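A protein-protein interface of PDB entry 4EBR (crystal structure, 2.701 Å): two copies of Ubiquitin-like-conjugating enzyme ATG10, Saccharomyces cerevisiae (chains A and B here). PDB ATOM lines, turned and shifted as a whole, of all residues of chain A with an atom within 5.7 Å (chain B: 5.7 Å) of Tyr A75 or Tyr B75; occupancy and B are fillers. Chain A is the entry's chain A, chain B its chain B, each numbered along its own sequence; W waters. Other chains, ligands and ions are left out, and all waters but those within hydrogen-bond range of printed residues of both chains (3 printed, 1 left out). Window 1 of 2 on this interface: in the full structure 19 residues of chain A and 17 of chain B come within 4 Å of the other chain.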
ATOM      1  N   GLY A   1      22.192  29.995  18.160  1.00  0.00           N
ATOM      2  CA  GLY A   1      21.258  30.825  18.903  1.00  0.00           C
ATOM      3  C   GLY A   1      21.643  31.001  20.365  1.00  0.00           C
ATOM      4  O   GLY A   1      22.503  30.278  20.882  1.00  0.00           O
ATOM      5  N   MET A   3      19.344  31.395  23.822  1.00  0.00           N
ATOM      6  CA  MET A   3      17.955  31.431  24.262  1.00  0.00           C
ATOM      7  C   MET A   3      17.689  32.394  25.401  1.00  0.00           C
ATOM      8  O   MET A   3      18.556  32.643  26.232  1.00  0.00           O
ATOM      9  CB  MET A   3      17.465  30.038  24.606  1.00  0.00           C
ATOM     10  CG  MET A   3      17.060  29.265  23.370  1.00  0.00           C
ATOM     11  SD  MET A   3      16.971  27.363  23.689  1.00  0.00           S
ATOM     12  CE  MET A   3      15.893  27.369  25.328  1.00  0.00           C
ATOM     13  N   TYR A  71       8.387  37.126  19.973  1.00  0.00           N
ATOM     14  CA  TYR A  71       9.127  36.095  20.647  1.00  0.00           C
ATOM     15  C   TYR A  71       8.756  34.752  20.042  1.00  0.00           C
ATOM     16  O   TYR A  71       7.585  34.462  19.831  1.00  0.00           O
ATOM     17  CB  TYR A  71       8.812  36.141  22.142  1.00  0.00           C
ATOM     18  CG  TYR A  71       9.516  35.077  22.951  1.00  0.00           C
ATOM     19  CD1 TYR A  71      10.845  35.232  23.327  1.00  0.00           C
ATOM     20  CD2 TYR A  71       8.851  33.918  23.342  1.00  0.00           C
ATOM     21  CE1 TYR A  71      11.509  34.254  24.068  1.00  0.00           C
ATOM     22  CE2 TYR A  71       9.495  32.933  24.097  1.00  0.00           C
ATOM     23  CZ  TYR A  71      10.829  33.102  24.455  1.00  0.00           C
ATOM     24  OH  TYR A  71      11.480  32.130  25.192  1.00  0.00           O
ATOM     25  N   SER A  72       9.738  33.923  19.739  1.00  0.00           N
ATOM     26  CA  SER A  72       9.413  32.562  19.310  1.00  0.00           C
ATOM     27  C   SER A  72       9.384  31.597  20.489  1.00  0.00           C
ATOM     28  O   SER A  72      10.403  31.381  21.157  1.00  0.00           O
ATOM     29  CB  SER A  72      10.438  32.067  18.309  1.00  0.00           C
ATOM     30  OG  SER A  72      10.233  30.697  18.067  1.00  0.00           O
ATOM     31  N   LYS A  73       8.234  30.996  20.744  1.00  0.00           N
ATOM     32  CA  LYS A  73       8.155  30.017  21.817  1.00  0.00           C
ATOM     33  C   LYS A  73       8.780  28.707  21.356  1.00  0.00           C
ATOM     34  O   LYS A  73       9.218  27.895  22.173  1.00  0.00           O
ATOM     35  CB  LYS A  73       6.710  29.799  22.253  1.00  0.00           C
ATOM     36  CG  LYS A  73       5.924  31.090  22.324  1.00  0.00           C
ATOM     37  CD  LYS A  73       5.152  31.265  23.626  1.00  0.00           C
ATOM     38  CE  LYS A  73       4.368  32.571  23.591  1.00  0.00           C
ATOM     39  NZ  LYS A  73       3.466  32.711  24.754  1.00  0.00           N
ATOM     40  N   VAL A  74       8.834  28.515  20.042  1.00  0.00           N
ATOM     41  CA  VAL A  74       9.441  27.322  19.483  1.00  0.00           C
ATOM     42  C   VAL A  74      10.932  27.310  19.757  1.00  0.00           C
ATOM     43  O   VAL A  74      11.488  26.289  20.163  1.00  0.00           O
ATOM     44  CB  VAL A  74       9.228  27.240  17.946  1.00  0.00           C
ATOM     45  CG1 VAL A  74       9.920  26.013  17.360  1.00  0.00           C
ATOM     46  CG2 VAL A  74       7.747  27.231  17.610  1.00  0.00           C
ATOM     47  N   TYR A  75      11.590  28.420  19.453  1.00  0.00           N
ATOM     48  CA  TYR A  75      13.033  28.500  19.601  1.00  0.00           C
ATOM     49  C   TYR A  75      13.540  29.221  20.855  1.00  0.00           C
ATOM     50  O   TYR A  75      14.750  29.226  21.105  1.00  0.00           O
ATOM     51  CB  TYR A  75      13.648  29.152  18.356  1.00  0.00           C
ATOM     52  CG  TYR A  75      13.373  28.421  17.078  1.00  0.00           C
ATOM     53  CD1 TYR A  75      13.806  27.110  16.896  1.00  0.00           C
ATOM     54  CD2 TYR A  75      12.680  29.036  16.035  1.00  0.00           C
ATOM     55  CE1 TYR A  75      13.538  26.419  15.715  1.00  0.00           C
ATOM     56  CE2 TYR A  75      12.404  28.343  14.844  1.00  0.00           C
ATOM     57  CZ  TYR A  75      12.851  27.044  14.692  1.00  0.00           C
ATOM     58  OH  TYR A  75      12.598  26.353  13.523  1.00  0.00           O
ATOM     59  N   ASN A  76      12.635  29.822  21.626  1.00  0.00           N
ATOM     60  CA  ASN A  76      13.020  30.700  22.755  1.00  0.00           C
ATOM     61  C   ASN A  76      14.006  31.802  22.407  1.00  0.00           C
ATOM     62  O   ASN A  76      15.001  32.001  23.092  1.00  0.00           O
ATOM     63  CB  ASN A  76      13.557  29.890  23.926  1.00  0.00           C
ATOM     64  CG  ASN A  76      12.562  28.898  24.410  1.00  0.00           C
ATOM     65  OD1 ASN A  76      12.797  27.686  24.375  1.00  0.00           O
ATOM     66  ND2 ASN A  76      11.407  29.394  24.835  1.00  0.00           N
ATOM     67  N   GLU A  77      13.714  32.501  21.323  1.00  0.00           N
ATOM     68  CA  GLU A  77      14.543  33.569  20.816  1.00  0.00           C
ATOM     69  C   GLU A  77      13.609  34.608  20.224  1.00  0.00           C
ATOM     70  O   GLU A  77      12.470  34.287  19.836  1.00  0.00           O
ATOM     71  CB  GLU A  77      15.483  33.034  19.741  1.00  0.00           C
ATOM     72  CG  GLU A  77      16.693  32.335  20.296  1.00  0.00           C
ATOM     73  CD  GLU A  77      17.712  31.956  19.216  1.00  0.00           C
ATOM     74  OE1 GLU A  77      18.243  30.816  19.287  1.00  0.00           O
ATOM     75  OE2 GLU A  77      17.981  32.794  18.313  1.00  0.00           O
ATOM     76  N   PRO A  78      14.067  35.862  20.166  1.00  0.00           N
ATOM     77  CA  PRO A  78      13.242  36.885  19.528  1.00  0.00           C
ATOM     78  C   PRO A  78      13.169  36.621  18.027  1.00  0.00           C
ATOM     79  O   PRO A  78      13.984  35.891  17.481  1.00  0.00           O
ATOM     80  CB  PRO A  78      14.018  38.183  19.787  1.00  0.00           C
ATOM     81  CG  PRO A  78      14.970  37.871  20.872  1.00  0.00           C
ATOM     82  CD  PRO A  78      15.316  36.420  20.698  1.00  0.00           C
ATOM     83  N   LEU A  79      12.131  37.150  17.394  1.00  0.00           N
ATOM     84  CA  LEU A  79      12.011  37.092  15.952  1.00  0.00           C
ATOM     85  C   LEU A  79      11.763  38.499  15.446  1.00  0.00           C
ATOM     86  O   LEU A  79      10.863  39.184  15.930  1.00  0.00           O
ATOM     87  CB  LEU A  79      10.860  36.172  15.544  1.00  0.00           C
ATOM     88  CG  LEU A  79      11.185  34.679  15.448  1.00  0.00           C
ATOM     89  CD1 LEU A  79      11.523  34.115  16.819  1.00  0.00           C
ATOM     90  CD2 LEU A  79      10.031  33.916  14.818  1.00  0.00           C
ATOM     91  N   SER A 131      10.999  36.840   7.924  1.00  0.00           N
ATOM     92  CA  SER A 131      11.799  36.664   9.118  1.00  0.00           C
ATOM     93  C   SER A 131      13.247  37.053   8.822  1.00  0.00           C
ATOM     94  O   SER A 131      13.883  36.480   7.940  1.00  0.00           O
ATOM     95  CB  SER A 131      11.749  35.198   9.471  1.00  0.00           C
ATOM     96  OG  SER A 131      12.699  34.918  10.457  1.00  0.00           O
ATOM     97  N   HIS A 133      17.119  37.397   9.714  1.00  0.00           N
ATOM     98  CA  HIS A 133      18.221  36.918  10.536  1.00  0.00           C
ATOM     99  C   HIS A 133      19.567  37.310   9.959  1.00  0.00           C
ATOM    100  O   HIS A 133      20.169  36.535   9.220  1.00  0.00           O
ATOM    101  CB  HIS A 133      18.195  35.397  10.625  1.00  0.00           C
ATOM    102  CG  HIS A 133      17.033  34.855  11.388  1.00  0.00           C
ATOM    103  ND1 HIS A 133      16.079  34.046  10.808  1.00  0.00           N
ATOM    104  CD2 HIS A 133      16.681  34.982  12.690  1.00  0.00           C
ATOM    105  CE1 HIS A 133      15.183  33.707  11.719  1.00  0.00           C
ATOM    106  NE2 HIS A 133      15.521  34.264  12.869  1.00  0.00           N
ATOM    107  N   GLY B   1      13.302  26.008  22.833  1.00  0.00           N
ATOM    108  CA  GLY B   1      14.327  25.483  21.952  1.00  0.00           C
ATOM    109  C   GLY B   1      15.357  24.577  22.605  1.00  0.00           C
ATOM    110  O   GLY B   1      15.348  24.346  23.810  1.00  0.00           O
ATOM    111  N   SER B   2      16.260  24.067  21.783  1.00  0.00           N
ATOM    112  CA  SER B   2      17.436  23.348  22.247  1.00  0.00           C
ATOM    113  C   SER B   2      18.648  23.767  21.386  1.00  0.00           C
ATOM    114  O   SER B   2      18.540  24.626  20.488  1.00  0.00           O
ATOM    115  CB  SER B   2      17.199  21.858  22.116  1.00  0.00           C
ATOM    116  OG  SER B   2      17.212  21.520  20.744  1.00  0.00           O
ATOM    117  N   MET B   3      19.809  23.192  21.668  1.00  0.00           N
ATOM    118  CA  MET B   3      20.984  23.430  20.847  1.00  0.00           C
ATOM    119  C   MET B   3      21.669  22.114  20.622  1.00  0.00           C
ATOM    120  O   MET B   3      21.913  21.366  21.559  1.00  0.00           O
ATOM    121  CB  MET B   3      21.963  24.361  21.537  1.00  0.00           C
ATOM    122  CG  MET B   3      21.379  25.701  21.988  1.00  0.00           C
ATOM    123  SD  MET B   3      20.853  26.918  20.551  1.00  0.00           S
ATOM    124  CE  MET B   3      20.091  28.327  21.648  1.00  0.00           C
ATOM    125  N   TYR B  71      19.376  21.236   9.149  1.00  0.00           N
ATOM    126  CA  TYR B  71      19.910  21.899  10.321  1.00  0.00           C
ATOM    127  C   TYR B  71      19.694  23.388  10.171  1.00  0.00           C
ATOM    128  O   TYR B  71      20.082  23.985   9.161  1.00  0.00           O
ATOM    129  CB  TYR B  71      21.413  21.610  10.476  1.00  0.00           C
ATOM    130  CG  TYR B  71      22.012  22.171  11.750  1.00  0.00           C
ATOM    131  CD1 TYR B  71      21.675  21.636  12.999  1.00  0.00           C
ATOM    132  CD2 TYR B  71      22.925  23.213  11.713  1.00  0.00           C
ATOM    133  CE1 TYR B  71      22.218  22.149  14.177  1.00  0.00           C
ATOM    134  CE2 TYR B  71      23.485  23.725  12.883  1.00  0.00           C
ATOM    135  CZ  TYR B  71      23.129  23.192  14.113  1.00  0.00           C
ATOM    136  OH  TYR B  71      23.683  23.719  15.271  1.00  0.00           O
ATOM    137  N   SER B  72      19.076  24.009  11.163  1.00  0.00           N
ATOM    138  CA  SER B  72      18.981  25.457  11.136  1.00  0.00           C
ATOM    139  C   SER B  72      20.247  26.026  11.740  1.00  0.00           C
ATOM    140  O   SER B  72      20.538  25.815  12.924  1.00  0.00           O
ATOM    141  CB  SER B  72      17.780  25.923  11.941  1.00  0.00           C
ATOM    142  OG  SER B  72      17.932  27.276  12.296  1.00  0.00           O
ATOM    143  N   LYS B  73      21.002  26.752  10.938  1.00  0.00           N
ATOM    144  CA  LYS B  73      22.211  27.379  11.441  1.00  0.00           C
ATOM    145  C   LYS B  73      21.899  28.617  12.282  1.00  0.00           C
ATOM    146  O   LYS B  73      22.738  29.058  13.061  1.00  0.00           O
ATOM    147  CB  LYS B  73      23.175  27.696  10.302  1.00  0.00           C
ATOM    148  CG  LYS B  73      23.829  26.448   9.721  1.00  0.00           C
ATOM    149  CD  LYS B  73      24.683  26.770   8.506  1.00  0.00           C
ATOM    150  CE  LYS B  73      25.044  25.508   7.736  1.00  0.00           C
ATOM    151  NZ  LYS B  73      25.704  25.815   6.429  1.00  0.00           N
ATOM    152  N   VAL B  74      20.692  29.164  12.149  1.00  0.00           N
ATOM    153  CA  VAL B  74      20.303  30.286  12.999  1.00  0.00           C
ATOM    154  C   VAL B  74      19.878  29.845  14.388  1.00  0.00           C
ATOM    155  O   VAL B  74      20.185  30.524  15.354  1.00  0.00           O
ATOM    156  CB  VAL B  74      19.199  31.173  12.373  1.00  0.00           C
ATOM    157  CG1 VAL B  74      19.791  32.098  11.364  1.00  0.00           C
ATOM    158  CG2 VAL B  74      18.220  30.332  11.677  1.00  0.00           C
ATOM    159  N   TYR B  75      19.129  28.749  14.494  1.00  0.00           N
ATOM    160  CA  TYR B  75      18.637  28.301  15.801  1.00  0.00           C
ATOM    161  C   TYR B  75      19.420  27.156  16.433  1.00  0.00           C
ATOM    162  O   TYR B  75      19.146  26.769  17.574  1.00  0.00           O
ATOM    163  CB  TYR B  75      17.142  27.943  15.730  1.00  0.00           C
ATOM    164  CG  TYR B  75      16.312  29.108  15.326  1.00  0.00           C
ATOM    165  CD1 TYR B  75      16.229  30.237  16.143  1.00  0.00           C
ATOM    166  CD2 TYR B  75      15.647  29.122  14.105  1.00  0.00           C
ATOM    167  CE1 TYR B  75      15.488  31.350  15.754  1.00  0.00           C
ATOM    168  CE2 TYR B  75      14.898  30.245  13.700  1.00  0.00           C
ATOM    169  CZ  TYR B  75      14.813  31.339  14.535  1.00  0.00           C
ATOM    170  OH  TYR B  75      14.086  32.436  14.136  1.00  0.00           O
ATOM    171  N   ASN B  76      20.376  26.622  15.682  1.00  0.00           N
ATOM    172  CA  ASN B  76      21.132  25.441  16.091  1.00  0.00           C
ATOM    173  C   ASN B  76      20.324  24.224  16.526  1.00  0.00           C
ATOM    174  O   ASN B  76      20.608  23.622  17.553  1.00  0.00           O
ATOM    175  CB  ASN B  76      22.158  25.819  17.149  1.00  0.00           C
ATOM    176  CG  ASN B  76      23.101  26.875  16.655  1.00  0.00           C
ATOM    177  OD1 ASN B  76      23.034  28.034  17.074  1.00  0.00           O
ATOM    178  ND2 ASN B  76      23.964  26.498  15.713  1.00  0.00           N
ATOM    179  N   GLU B  77      19.341  23.865  15.717  1.00  0.00           N
ATOM    180  CA  GLU B  77      18.405  22.794  16.000  1.00  0.00           C
ATOM    181  C   GLU B  77      18.044  22.170  14.675  1.00  0.00           C
ATOM    182  O   GLU B  77      18.142  22.836  13.628  1.00  0.00           O
ATOM    183  CB  GLU B  77      17.136  23.381  16.572  1.00  0.00           C
ATOM    184  CG  GLU B  77      17.122  23.515  18.047  1.00  0.00           C
ATOM    185  CD  GLU B  77      16.106  24.547  18.489  1.00  0.00           C
ATOM    186  OE1 GLU B  77      16.504  25.567  19.122  1.00  0.00           O
ATOM    187  OE2 GLU B  77      14.914  24.334  18.168  1.00  0.00           O
ATOM    188  N   PRO B  78      17.592  20.910  14.693  1.00  0.00           N
ATOM    189  CA  PRO B  78      17.108  20.355  13.428  1.00  0.00           C
ATOM    190  C   PRO B  78      15.888  21.143  12.959  1.00  0.00           C
ATOM    191  O   PRO B  78      15.192  21.780  13.751  1.00  0.00           O
ATOM    192  CB  PRO B  78      16.692  18.925  13.803  1.00  0.00           C
ATOM    193  CG  PRO B  78      17.313  18.670  15.157  1.00  0.00           C
ATOM    194  CD  PRO B  78      17.317  20.012  15.819  1.00  0.00           C
ATOM    195  N   LEU B  79      15.640  21.118  11.667  1.00  0.00           N
ATOM    196  CA  LEU B  79      14.482  21.794  11.127  1.00  0.00           C
ATOM    197  C   LEU B  79      13.827  20.779  10.188  1.00  0.00           C
ATOM    198  O   LEU B  79      14.462  20.314   9.255  1.00  0.00           O
ATOM    199  CB  LEU B  79      14.929  23.046  10.388  1.00  0.00           C
ATOM    200  CG  LEU B  79      13.849  23.927   9.784  1.00  0.00           C
ATOM    201  CD1 LEU B  79      12.832  24.322  10.844  1.00  0.00           C
ATOM    202  CD2 LEU B  79      14.490  25.165   9.144  1.00  0.00           C
ATOM    203  N   SER B 131       7.438  24.449   7.835  1.00  0.00           N
ATOM    204  CA  SER B 131       8.239  24.136   9.000  1.00  0.00           C
ATOM    205  C   SER B 131       7.384  23.302   9.964  1.00  0.00           C
ATOM    206  O   SER B 131       6.348  23.753  10.436  1.00  0.00           O
ATOM    207  CB  SER B 131       8.627  25.453   9.657  1.00  0.00           C
ATOM    208  OG  SER B 131       9.606  25.237  10.646  1.00  0.00           O
ATOM    209  N   HIS B 133       6.495  21.784  13.468  1.00  0.00           N
ATOM    210  CA  HIS B 133       6.808  21.983  14.897  1.00  0.00           C
ATOM    211  C   HIS B 133       5.714  21.502  15.843  1.00  0.00           C
ATOM    212  O   HIS B 133       5.059  22.319  16.474  1.00  0.00           O
ATOM    213  CB  HIS B 133       7.009  23.460  15.196  1.00  0.00           C
ATOM    214  CG  HIS B 133       8.272  24.017  14.642  1.00  0.00           C
ATOM    215  ND1 HIS B 133       9.515  23.565  15.033  1.00  0.00           N
ATOM    216  CD2 HIS B 133       8.492  25.001  13.739  1.00  0.00           C
ATOM    217  CE1 HIS B 133      10.448  24.239  14.382  1.00  0.00           C
ATOM    218  NE2 HIS B 133       9.854  25.116  13.592  1.00  0.00           N
HETATM  219  O   HOH W   1      19.727  33.059  16.415  1.00  0.00           O
HETATM  220  O   HOH W   2      12.272  32.356  11.649  1.00  0.00           O
HETATM  221  O   HOH W   3      11.232  27.883  11.446  1.00  0.00           O
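The backbone NH (N) of Gly A1 sits at hydrogen-bond distance from the backbone carbonyl oxygen (O) of Val B74. O of Val A74 lies within hydrogen-bond range of N of Gly B1, at 3.2 Å. The side-chain hydroxyl of Tyr A75 is in hydrogen-bond range of a ring nitrogen (NE2) of His B133, at 3.0 Å. NE2 of His A133 sits at hydrogen-bond distance from OH of Tyr B75 (2.6 Å). The side-chain sulfur of Met B3 sits close to the backbone carbonyl oxygen of Gly A1, at 3.8 Å. N of Gly A1 sits close to OD1 of Asn B76. O of Gly B1 lies close to SD of Met A3 (3.4 Å). The side-chain amide oxygen (OD1) of Asn A76 lies close to the backbone NH (N) of Gly B1, 2.3 Å away.
Tyr A75 touches five residues of chain B. Of the printed residues of chain B, Met A3 touches Gly B1 (3.4 Å), Ser B2 (3.9 Å) and Met B3 (3.6 Å). Of the printed residues of chain B, Val A74 touches Gly B1 (3.2 Å) and His B133 (3.4 Å). The nearest residue of chain B that does not touch Tyr A75 is Ser B131 (4.3 Å). The nearest residue of chain A that does not touch Tyr B75 is Gly A1 (4.3 Å).
Hydrophobic or aromatic side chains of chain A that line the printed part of chain B: Met A3, Val A74, Tyr A75, Leu A79 and His A133. Printed residues of chain B that touch a printed residue of chain A: Gly B1, Ser B2, Met B3, Val B74, Tyr B75, Asn B76, Glu B77, Leu B79 and His B133. Hydrophobic or aromatic side chains of chain B within 4 Å of the printed part of chain A: Met B3, Val B74, Tyr B75, Leu B79 and His B133.
Water W1 bridges OE2 of Glu A77 (2.6 Å) and O of Val B74 (2.8 Å). Water W2 lies within hydrogen-bond range of OG of Ser A131 (2.9 Å) and OH of Tyr B75 (3.1 Å). Water W3 lies within hydrogen-bond range of OH of Tyr A75 (2.9 Å) and OG of Ser B131 (3.2 Å).
Gly A1 touches Met B3, and with the chains exchanged Met A3 touches Gly B1. Tyr A75 touches Gly B1, but with the chains exchanged Gly A1 does not touch Tyr B75 (4.3 Å). Tyr A75 touches Leu B79, and with the chains exchanged Leu A79 touches Tyr B75. Glu A77 touches Met B3, but with the chains exchanged Met A3 does not touch Glu B77 (4.9 Å). Positions printed for both chains: 1, 3, 71, 72, 73, 74, 75, 76, 77, 78, 79, 131 and 133. Of the 19 pairs that touch across the chains among the printed residues, 16 have their exchanged pair printed and touching as well.
The side-chain hydroxyl (OH) of Tyr A71 sits at hydrogen-bond distance from the side-chain amide nitrogen (ND2) of Asn A76. The backbone NH of Val A74 lies close to the side-chain hydroxyl of Ser A72. OG of Ser A72 lies within hydrogen-bond range of N of Tyr A75 (3.0 Å). The side-chain hydroxyl of Tyr B71 is in hydrogen-bond range of the side-chain amide nitrogen of Asn B76 (2.8 Å). The backbone NH (N) of Tyr B75 sits at hydrogen-bond distance from the side-chain hydroxyl (OG) of Ser B72, 2.9 Å away. NE2 of His B133 lies within hydrogen-bond range of OG of Ser B131 (3.0 Å).
SD of Met A3 touches N of Ser B2 (3.9 Å). Met A3 touches Met B3. CG1 of Val A74 touches ND1 of His B133, at 3.4 Å. C of Tyr A75 touches N of Gly B1 (3.8 Å). Tyr B75 touches Tyr A75. Glu B77 touches Tyr A75 (OE2 to CD1, 3.2 Å). Leu B79 touches Tyr A75 (CD1 to OH, 3.4 Å). Glu A77 touches Tyr B75 (OE1 to CD1, 3.8 Å). Leu A79 touches Tyr B75 (CG to OH, 3.9 Å). CG1 of Val B74 touches CB of His A133 (3.7 Å).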
